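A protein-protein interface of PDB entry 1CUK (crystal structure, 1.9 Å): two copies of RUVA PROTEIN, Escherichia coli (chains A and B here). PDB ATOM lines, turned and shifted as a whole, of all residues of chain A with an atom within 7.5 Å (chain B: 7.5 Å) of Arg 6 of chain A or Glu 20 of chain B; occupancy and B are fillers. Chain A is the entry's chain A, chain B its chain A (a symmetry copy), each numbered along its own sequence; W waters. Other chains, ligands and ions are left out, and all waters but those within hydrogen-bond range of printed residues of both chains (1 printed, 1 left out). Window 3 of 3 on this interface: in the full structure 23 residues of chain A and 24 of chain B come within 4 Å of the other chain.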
ATOM      1  N   ARG A   4       0.676  -8.993   9.026  1.00  0.00           N
ATOM      2  CA  ARG A   4       1.090 -10.306   9.472  1.00  0.00           C
ATOM      3  C   ARG A   4       0.020 -11.015  10.257  1.00  0.00           C
ATOM      4  O   ARG A   4      -0.750 -10.405  10.935  1.00  0.00           O
ATOM      5  CB  ARG A   4       2.335 -10.224  10.372  1.00  0.00           C
ATOM      6  CG  ARG A   4       3.099 -11.566  10.450  1.00  0.00           C
ATOM      7  CD  ARG A   4       4.246 -11.502  11.444  1.00  0.00           C
ATOM      8  NE  ARG A   4       3.734 -11.692  12.784  1.00  0.00           N
ATOM      9  CZ  ARG A   4       4.426 -12.064  13.873  1.00  0.00           C
ATOM     10  NH1 ARG A   4       5.723 -12.300  13.848  1.00  0.00           N
ATOM     11  NH2 ARG A   4       3.772 -12.204  15.027  1.00  0.00           N
ATOM     12  N   LEU A   5      -0.021 -12.343  10.139  1.00  0.00           N
ATOM     13  CA  LEU A   5      -0.999 -13.112  10.879  1.00  0.00           C
ATOM     14  C   LEU A   5      -0.251 -14.235  11.621  1.00  0.00           C
ATOM     15  O   LEU A   5       0.656 -14.825  11.071  1.00  0.00           O
ATOM     16  CB  LEU A   5      -2.086 -13.783   9.947  1.00  0.00           C
ATOM     17  CG  LEU A   5      -3.525 -13.205   9.871  1.00  0.00           C
ATOM     18  CD1 LEU A   5      -3.759 -11.817  10.453  1.00  0.00           C
ATOM     19  CD2 LEU A   5      -4.149 -13.391   8.493  1.00  0.00           C
ATOM     20  N   ARG A   6      -0.695 -14.494  12.851  1.00  0.00           N
ATOM     21  CA  ARG A   6      -0.140 -15.541  13.712  1.00  0.00           C
ATOM     22  C   ARG A   6      -1.296 -16.336  14.239  1.00  0.00           C
ATOM     23  O   ARG A   6      -2.079 -15.807  14.953  1.00  0.00           O
ATOM     24  CB  ARG A   6       0.654 -14.955  14.859  1.00  0.00           C
ATOM     25  CG  ARG A   6       1.256 -16.105  15.641  1.00  0.00           C
ATOM     26  CD  ARG A   6       2.276 -15.687  16.691  1.00  0.00           C
ATOM     27  NE  ARG A   6       1.762 -14.657  17.560  1.00  0.00           N
ATOM     28  CZ  ARG A   6       0.968 -14.847  18.603  1.00  0.00           C
ATOM     29  NH1 ARG A   6       0.565 -16.076  18.979  1.00  0.00           N
ATOM     30  NH2 ARG A   6       0.553 -13.791  19.328  1.00  0.00           N
ATOM     31  N   GLY A   7      -1.468 -17.586  13.835  1.00  0.00           N
ATOM     32  CA  GLY A   7      -2.610 -18.347  14.322  1.00  0.00           C
ATOM     33  C   GLY A   7      -2.535 -19.812  13.949  1.00  0.00           C
ATOM     34  O   GLY A   7      -1.524 -20.299  13.473  1.00  0.00           O
ATOM     35  N   ILE A   8      -3.615 -20.543  14.133  1.00  0.00           N
ATOM     36  CA  ILE A   8      -3.634 -21.967  13.828  1.00  0.00           C
ATOM     37  C   ILE A   8      -4.206 -22.328  12.416  1.00  0.00           C
ATOM     38  O   ILE A   8      -5.287 -21.864  12.061  1.00  0.00           O
ATOM     39  CB  ILE A   8      -4.476 -22.666  14.897  1.00  0.00           C
ATOM     40  CG1 ILE A   8      -3.890 -22.353  16.262  1.00  0.00           C
ATOM     41  CG2 ILE A   8      -4.466 -24.177  14.660  1.00  0.00           C
ATOM     42  CD1 ILE A   8      -2.451 -22.864  16.392  1.00  0.00           C
ATOM     43  N   ILE A  19      -6.571 -19.601   8.329  1.00  0.00           N
ATOM     44  CA  ILE A  19      -5.844 -19.394   9.589  1.00  0.00           C
ATOM     45  C   ILE A  19      -6.729 -18.780  10.666  1.00  0.00           C
ATOM     46  O   ILE A  19      -7.306 -17.719  10.436  1.00  0.00           O
ATOM     47  CB  ILE A  19      -4.613 -18.526   9.380  1.00  0.00           C
ATOM     48  CG1 ILE A  19      -3.827 -19.046   8.219  1.00  0.00           C
ATOM     49  CG2 ILE A  19      -3.716 -18.506  10.629  1.00  0.00           C
ATOM     50  CD1 ILE A  19      -2.402 -18.510   8.224  1.00  0.00           C
ATOM     51  N   GLU A  20      -6.877 -19.510  11.813  1.00  0.00           N
ATOM     52  CA  GLU A  20      -7.683 -19.070  12.922  1.00  0.00           C
ATOM     53  C   GLU A  20      -6.945 -18.240  13.879  1.00  0.00           C
ATOM     54  O   GLU A  20      -5.948 -18.633  14.421  1.00  0.00           O
ATOM     55  CB  GLU A  20      -8.461 -20.152  13.621  1.00  0.00           C
ATOM     56  CG  GLU A  20      -9.640 -19.463  14.290  1.00  0.00           C
ATOM     57  CD  GLU A  20     -10.539 -20.371  15.042  1.00  0.00           C
ATOM     58  OE1 GLU A  20     -10.206 -20.944  16.016  1.00  0.00           O
ATOM     59  OE2 GLU A  20     -11.716 -20.488  14.505  1.00  0.00           O
ATOM     60  N   VAL A  21      -7.433 -17.053  14.028  1.00  0.00           N
ATOM     61  CA  VAL A  21      -6.835 -16.142  14.878  1.00  0.00           C
ATOM     62  C   VAL A  21      -7.845 -15.648  15.864  1.00  0.00           C
ATOM     63  O   VAL A  21      -8.681 -14.814  15.539  1.00  0.00           O
ATOM     64  CB  VAL A  21      -6.266 -14.946  14.091  1.00  0.00           C
ATOM     65  CG1 VAL A  21      -5.618 -13.985  15.080  1.00  0.00           C
ATOM     66  CG2 VAL A  21      -5.264 -15.398  13.002  1.00  0.00           C
ATOM     67  N   GLY A  22      -7.785 -16.161  17.087  1.00  0.00           N
ATOM     68  CA  GLY A  22      -8.701 -15.726  18.119  1.00  0.00           C
ATOM     69  C   GLY A  22     -10.174 -15.873  17.714  1.00  0.00           C
ATOM     70  O   GLY A  22     -10.980 -14.994  17.998  1.00  0.00           O
ATOM     71  N   GLU A  44       0.520 -24.008  14.630  1.00  0.00           N
ATOM     72  CA  GLU A  44       0.697 -22.586  14.520  1.00  0.00           C
ATOM     73  C   GLU A  44       1.534 -22.205  13.344  1.00  0.00           C
ATOM     74  O   GLU A  44       2.579 -22.822  13.079  1.00  0.00           O
ATOM     75  CB  GLU A  44       1.371 -21.977  15.783  1.00  0.00           C
ATOM     76  CG  GLU A  44       1.430 -20.440  15.742  1.00  0.00           C
ATOM     77  CD  GLU A  44       2.086 -19.821  16.946  1.00  0.00           C
ATOM     78  OE1 GLU A  44       1.213 -19.601  17.905  1.00  0.00           O
ATOM     79  OE2 GLU A  44       3.291 -19.532  17.006  1.00  0.00           O
ATOM     80  N   ALA A  45       1.072 -21.133  12.647  1.00  0.00           N
ATOM     81  CA  ALA A  45       1.767 -20.591  11.515  1.00  0.00           C
ATOM     82  C   ALA A  45       1.866 -19.060  11.590  1.00  0.00           C
ATOM     83  O   ALA A  45       1.048 -18.376  12.190  1.00  0.00           O
ATOM     84  CB  ALA A  45       1.112 -21.004  10.211  1.00  0.00           C
ATOM     85  N   ILE A  46       2.909 -18.551  10.976  1.00  0.00           N
ATOM     86  CA  ILE A  46       3.135 -17.118  10.889  1.00  0.00           C
ATOM     87  C   ILE A  46       3.216 -16.768   9.402  1.00  0.00           C
ATOM     88  O   ILE A  46       4.049 -17.332   8.679  1.00  0.00           O
ATOM     89  CB  ILE A  46       4.375 -16.617  11.626  1.00  0.00           C
ATOM     90  CG1 ILE A  46       4.084 -16.650  13.106  1.00  0.00           C
ATOM     91  CG2 ILE A  46       4.652 -15.171  11.218  1.00  0.00           C
ATOM     92  CD1 ILE A  46       5.285 -16.336  13.936  1.00  0.00           C
ATOM     93  N   VAL A  47       2.342 -15.861   8.947  1.00  0.00           N
ATOM     94  CA  VAL A  47       2.372 -15.468   7.529  1.00  0.00           C
ATOM     95  C   VAL A  47       2.351 -13.951   7.358  1.00  0.00           C
ATOM     96  O   VAL A  47       1.661 -13.231   8.091  1.00  0.00           O
ATOM     97  CB  VAL A  47       1.376 -16.193   6.600  1.00  0.00           C
ATOM     98  CG1 VAL A  47       1.340 -17.696   6.856  1.00  0.00           C
ATOM     99  CG2 VAL A  47       0.015 -15.620   6.782  1.00  0.00           C
ATOM    100  N   LEU B   5      -4.445   1.573  19.187  1.00  0.00           N
ATOM    101  CA  LEU B   5      -3.971   0.206  19.197  1.00  0.00           C
ATOM    102  C   LEU B   5      -3.067   0.031  20.431  1.00  0.00           C
ATOM    103  O   LEU B   5      -2.298   0.914  20.750  1.00  0.00           O
ATOM    104  CB  LEU B   5      -3.122  -0.158  17.914  1.00  0.00           C
ATOM    105  CG  LEU B   5      -3.728  -1.040  16.790  1.00  0.00           C
ATOM    106  CD1 LEU B   5      -5.235  -1.264  16.806  1.00  0.00           C
ATOM    107  CD2 LEU B   5      -3.192  -0.669  15.412  1.00  0.00           C
ATOM    108  N   ARG B   6      -3.192  -1.137  21.062  1.00  0.00           N
ATOM    109  CA  ARG B   6      -2.405  -1.514  22.239  1.00  0.00           C
ATOM    110  C   ARG B   6      -1.854  -2.884  21.980  1.00  0.00           C
ATOM    111  O   ARG B   6      -2.605  -3.793  21.873  1.00  0.00           O
ATOM    112  CB  ARG B   6      -3.250  -1.522  23.494  1.00  0.00           C
ATOM    113  CG  ARG B   6      -2.339  -1.837  24.663  1.00  0.00           C
ATOM    114  CD  ARG B   6      -2.984  -1.655  26.030  1.00  0.00           C
ATOM    115  NE  ARG B   6      -4.245  -2.350  26.128  1.00  0.00           N
ATOM    116  CZ  ARG B   6      -4.400  -3.642  26.376  1.00  0.00           C
ATOM    117  NH1 ARG B   6      -3.351  -4.459  26.592  1.00  0.00           N
ATOM    118  NH2 ARG B   6      -5.639  -4.167  26.432  1.00  0.00           N
ATOM    119  N   GLY B   7      -0.552  -3.040  21.795  1.00  0.00           N
ATOM    120  CA  GLY B   7      -0.021  -4.367  21.510  1.00  0.00           C
ATOM    121  C   GLY B   7       1.491  -4.409  21.550  1.00  0.00           C
ATOM    122  O   GLY B   7       2.145  -3.472  21.975  1.00  0.00           O
ATOM    123  N   ILE B   8       2.082  -5.491  21.086  1.00  0.00           N
ATOM    124  CA  ILE B   8       3.531  -5.637  21.105  1.00  0.00           C
ATOM    125  C   ILE B   8       4.248  -5.245  19.769  1.00  0.00           C
ATOM    126  O   ILE B   8       3.847  -5.712  18.705  1.00  0.00           O
ATOM    127  CB  ILE B   8       3.852  -7.097  21.430  1.00  0.00           C
ATOM    128  CG1 ILE B   8       3.195  -7.459  22.750  1.00  0.00           C
ATOM    129  CG2 ILE B   8       5.366  -7.284  21.532  1.00  0.00           C
ATOM    130  CD1 ILE B   8       3.723  -6.596  23.902  1.00  0.00           C
ATOM    131  N   ILE B   9       5.311  -4.426  19.854  1.00  0.00           N
ATOM    132  CA  ILE B   9       6.082  -4.032  18.685  1.00  0.00           C
ATOM    133  C   ILE B   9       6.835  -5.259  18.202  1.00  0.00           C
ATOM    134  O   ILE B   9       7.679  -5.776  18.917  1.00  0.00           O
ATOM    135  CB  ILE B   9       7.109  -2.889  18.978  1.00  0.00           C
ATOM    136  CG1 ILE B   9       6.458  -1.613  19.478  1.00  0.00           C
ATOM    137  CG2 ILE B   9       7.929  -2.548  17.722  1.00  0.00           C
ATOM    138  CD1 ILE B   9       5.473  -1.035  18.476  1.00  0.00           C
ATOM    139  N   ILE B  10       6.505  -5.713  17.004  1.00  0.00           N
ATOM    140  CA  ILE B  10       7.112  -6.856  16.402  1.00  0.00           C
ATOM    141  C   ILE B  10       8.299  -6.440  15.532  1.00  0.00           C
ATOM    142  O   ILE B  10       9.313  -7.134  15.495  1.00  0.00           O
ATOM    143  CB  ILE B  10       6.119  -7.556  15.480  1.00  0.00           C
ATOM    144  CG1 ILE B  10       4.900  -8.072  16.191  1.00  0.00           C
ATOM    145  CG2 ILE B  10       6.810  -8.700  14.760  1.00  0.00           C
ATOM    146  CD1 ILE B  10       5.269  -9.165  17.153  1.00  0.00           C
ATOM    147  N   GLU B  11       8.166  -5.344  14.781  1.00  0.00           N
ATOM    148  CA  GLU B  11       9.265  -4.879  13.915  1.00  0.00           C
ATOM    149  C   GLU B  11       9.151  -3.444  13.670  1.00  0.00           C
ATOM    150  O   GLU B  11       8.072  -2.901  13.633  1.00  0.00           O
ATOM    151  CB  GLU B  11       9.228  -5.435  12.496  1.00  0.00           C
ATOM    152  CG  GLU B  11       9.825  -6.807  12.265  1.00  0.00           C
ATOM    153  CD  GLU B  11       9.233  -7.403  11.018  1.00  0.00           C
ATOM    154  OE1 GLU B  11       8.871  -6.440  10.147  1.00  0.00           O
ATOM    155  OE2 GLU B  11       9.040  -8.586  10.867  1.00  0.00           O
ATOM    156  N   VAL B  17       5.809   0.553  11.354  1.00  0.00           N
ATOM    157  CA  VAL B  17       5.951  -0.233  12.591  1.00  0.00           C
ATOM    158  C   VAL B  17       4.875  -1.307  12.548  1.00  0.00           C
ATOM    159  O   VAL B  17       3.747  -1.023  12.151  1.00  0.00           O
ATOM    160  CB  VAL B  17       5.973   0.564  13.937  1.00  0.00           C
ATOM    161  CG1 VAL B  17       4.640   1.296  14.199  1.00  0.00           C
ATOM    162  CG2 VAL B  17       6.216  -0.409  15.080  1.00  0.00           C
ATOM    163  N   LEU B  18       5.221  -2.529  12.909  1.00  0.00           N
ATOM    164  CA  LEU B  18       4.285  -3.628  12.918  1.00  0.00           C
ATOM    165  C   LEU B  18       3.974  -3.933  14.373  1.00  0.00           C
ATOM    166  O   LEU B  18       4.901  -4.287  15.109  1.00  0.00           O
ATOM    167  CB  LEU B  18       4.956  -4.844  12.274  1.00  0.00           C
ATOM    168  CG  LEU B  18       4.049  -6.051  12.117  1.00  0.00           C
ATOM    169  CD1 LEU B  18       2.893  -5.762  11.166  1.00  0.00           C
ATOM    170  CD2 LEU B  18       4.899  -7.158  11.550  1.00  0.00           C
ATOM    171  N   ILE B  19       2.673  -3.773  14.760  1.00  0.00           N
ATOM    172  CA  ILE B  19       2.155  -3.988  16.118  1.00  0.00           C
ATOM    173  C   ILE B  19       1.215  -5.185  16.188  1.00  0.00           C
ATOM    174  O   ILE B  19       0.234  -5.222  15.448  1.00  0.00           O
ATOM    175  CB  ILE B  19       1.448  -2.749  16.643  1.00  0.00           C
ATOM    176  CG1 ILE B  19       2.317  -1.551  16.428  1.00  0.00           C
ATOM    177  CG2 ILE B  19       1.122  -2.876  18.140  1.00  0.00           C
ATOM    178  CD1 ILE B  19       1.878  -0.380  17.296  1.00  0.00           C
ATOM    179  N   GLU B  20       1.580  -6.189  17.042  1.00  0.00           N
ATOM    180  CA  GLU B  20       0.802  -7.387  17.219  1.00  0.00           C
ATOM    181  C   GLU B  20      -0.226  -7.260  18.258  1.00  0.00           C
ATOM    182  O   GLU B  20       0.049  -6.958  19.386  1.00  0.00           O
ATOM    183  CB  GLU B  20       1.598  -8.653  17.389  1.00  0.00           C
ATOM    184  CG  GLU B  20       0.687  -9.790  16.955  1.00  0.00           C
ATOM    185  CD  GLU B  20       1.295 -11.138  17.051  1.00  0.00           C
ATOM    186  OE1 GLU B  20       1.585 -11.642  18.076  1.00  0.00           O
ATOM    187  OE2 GLU B  20       1.497 -11.694  15.894  1.00  0.00           O
ATOM    188  N   VAL B  21      -1.430  -7.443  17.826  1.00  0.00           N
ATOM    189  CA  VAL B  21      -2.512  -7.333  18.679  1.00  0.00           C
ATOM    190  C   VAL B  21      -3.319  -8.592  18.621  1.00  0.00           C
ATOM    191  O   VAL B  21      -4.068  -8.811  17.679  1.00  0.00           O
ATOM    192  CB  VAL B  21      -3.404  -6.140  18.286  1.00  0.00           C
ATOM    193  CG1 VAL B  21      -4.571  -6.070  19.263  1.00  0.00           C
ATOM    194  CG2 VAL B  21      -2.610  -4.813  18.257  1.00  0.00           C
ATOM    195  N   GLY B  22      -3.171  -9.441  19.631  1.00  0.00           N
ATOM    196  CA  GLY B  22      -3.930 -10.672  19.680  1.00  0.00           C
ATOM    197  C   GLY B  22      -3.751 -11.536  18.424  1.00  0.00           C
ATOM    198  O   GLY B  22      -4.716 -12.110  17.932  1.00  0.00           O
ATOM    199  N   GLY B  23      -2.527 -11.596  17.909  1.00  0.00           N
ATOM    200  CA  GLY B  23      -2.231 -12.403  16.735  1.00  0.00           C
ATOM    201  C   GLY B  23      -2.350 -11.635  15.407  1.00  0.00           C
ATOM    202  O   GLY B  23      -1.912 -12.123  14.394  1.00  0.00           O
ATOM    203  N   VAL B  24      -2.963 -10.473  15.432  1.00  0.00           N
ATOM    204  CA  VAL B  24      -3.100  -9.679  14.226  1.00  0.00           C
ATOM    205  C   VAL B  24      -2.002  -8.613  14.200  1.00  0.00           C
ATOM    206  O   VAL B  24      -1.910  -7.786  15.086  1.00  0.00           O
ATOM    207  CB  VAL B  24      -4.494  -9.080  14.045  1.00  0.00           C
ATOM    208  CG1 VAL B  24      -4.541  -8.275  12.735  1.00  0.00           C
ATOM    209  CG2 VAL B  24      -5.540 -10.181  14.013  1.00  0.00           C
ATOM    210  N   GLY B  25      -1.141  -8.682  13.182  1.00  0.00           N
ATOM    211  CA  GLY B  25      -0.057  -7.744  13.045  1.00  0.00           C
ATOM    212  C   GLY B  25      -0.507  -6.552  12.184  1.00  0.00           C
ATOM    213  O   GLY B  25      -0.699  -6.671  10.996  1.00  0.00           O
ATOM    214  N   TYR B  26      -0.692  -5.417  12.809  1.00  0.00           N
ATOM    215  CA  TYR B  26      -1.124  -4.186  12.149  1.00  0.00           C
ATOM    216  C   TYR B  26       0.044  -3.321  11.722  1.00  0.00           C
ATOM    217  O   TYR B  26       0.931  -3.032  12.509  1.00  0.00           O
ATOM    218  CB  TYR B  26      -2.009  -3.299  13.058  1.00  0.00           C
ATOM    219  CG  TYR B  26      -3.382  -3.864  13.255  1.00  0.00           C
ATOM    220  CD1 TYR B  26      -4.383  -3.607  12.314  1.00  0.00           C
ATOM    221  CD2 TYR B  26      -3.690  -4.672  14.358  1.00  0.00           C
ATOM    222  CE1 TYR B  26      -5.665  -4.128  12.456  1.00  0.00           C
ATOM    223  CE2 TYR B  26      -4.974  -5.202  14.519  1.00  0.00           C
ATOM    224  CZ  TYR B  26      -5.954  -4.923  13.566  1.00  0.00           C
ATOM    225  OH  TYR B  26      -7.203  -5.435  13.709  1.00  0.00           O
ATOM    226  N   ALA B  45       3.315  -1.223  23.274  1.00  0.00           N
ATOM    227  CA  ALA B  45       3.153   0.133  22.833  1.00  0.00           C
ATOM    228  C   ALA B  45       1.672   0.509  22.684  1.00  0.00           C
ATOM    229  O   ALA B  45       0.803  -0.320  22.444  1.00  0.00           O
ATOM    230  CB  ALA B  45       3.885   0.383  21.528  1.00  0.00           C
HETATM  231  O   HOH W   1       4.811 -12.881  17.915  1.00  0.00           O
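Hydrophobic or aromatic side chains of chain A that line the printed part of chain B: Val 21.
Hydrophobic or aromatic side chains of chain B that line the printed part of chain A: Ile 10 and Val 24.
The backbone NH (N) of Leu 5 of chain A sits at hydrogen-bond distance from the backbone carbonyl oxygen (O) of Val 47 of chain A, at 2.8 Å.
NH1 of Arg 6 of chain A lies within salt-bridge range of OE1 of Glu 44 of chain A (3.7 Å).
The backbone carbonyl oxygen (O) of Ile 8 of chain B is in hydrogen-bond range of the backbone NH (N) of Glu 20 of chain B (2.9 Å).
O of Leu 18 of chain B is in hydrogen-bond range of N of Ile 10 of chain B, at 2.9 Å.
Arg 6 of chain A touches Glu 20 of chain B, but with the chains exchanged Glu 20 of chain A does not touch Arg 6 of chain B (16.9 Å).
Val 21 of chain A touches Gly 22 of chain B, but with the chains exchanged Gly 22 of chain A does not touch Val 21 of chain B (8.3 Å).
Of the 9 pairs that touch across the chains among the printed residues, none has its exchanged pair printed and touching as well.
Arg 6 of chain A touches two residues of chain B.
Glu 20 of chain B touches two residues of chain A.
Printed residues of chain B within 4 Å of Arg 4 of chain A: Ile 10, Glu 20, Val 24 and Gly 25.
Printed residues of chain B within 4 Å of Val 21 of chain A: Gly 22 and Val 24.
Printed residues of chain A within 4 Å of Ile 10 of chain B: Arg 4.
The nearest residue of chain B that does not touch Arg 6 of chain A is Gly 22 of chain B (4.9 Å).
The nearest residue of chain A that does not touch Glu 20 of chain B is Leu 5 of chain A (5.3 Å).
Water W1 lies within hydrogen-bond range of NH2 of Arg 4 of chain A (3.1 Å) and OE1 of Glu 20 of chain B (3.5 Å).
Arg 4 of chain A touches Ile 10 of chain B.
C of Val 24 of chain B touches O of Arg 4 of chain A (3.9 Å).
CA of Leu 5 of chain A touches O of Gly 23 of chain B, 3.8 Å away.
Gly 22 of chain B touches Val 21 of chain A (O to CG1, 3.5 Å).
Val 21 of chain A touches Val 24 of chain B.
The side-chain carboxylate of Glu 20 of chain B lies within salt-bridge range of the guanidinium group of Arg 4 of chain A, at 2.5 Å.
N of Gly 25 of chain B is in hydrogen-bond range of O of Arg 4 of chain A, at 2.9 Å.
NH2 of Arg 6 of chain A lies within salt-bridge range of OE1 of Glu 20 of chain B.
N of Arg 6 of chain A is in hydrogen-bond range of O of Gly 23 of chain B, 3.1 Å away.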
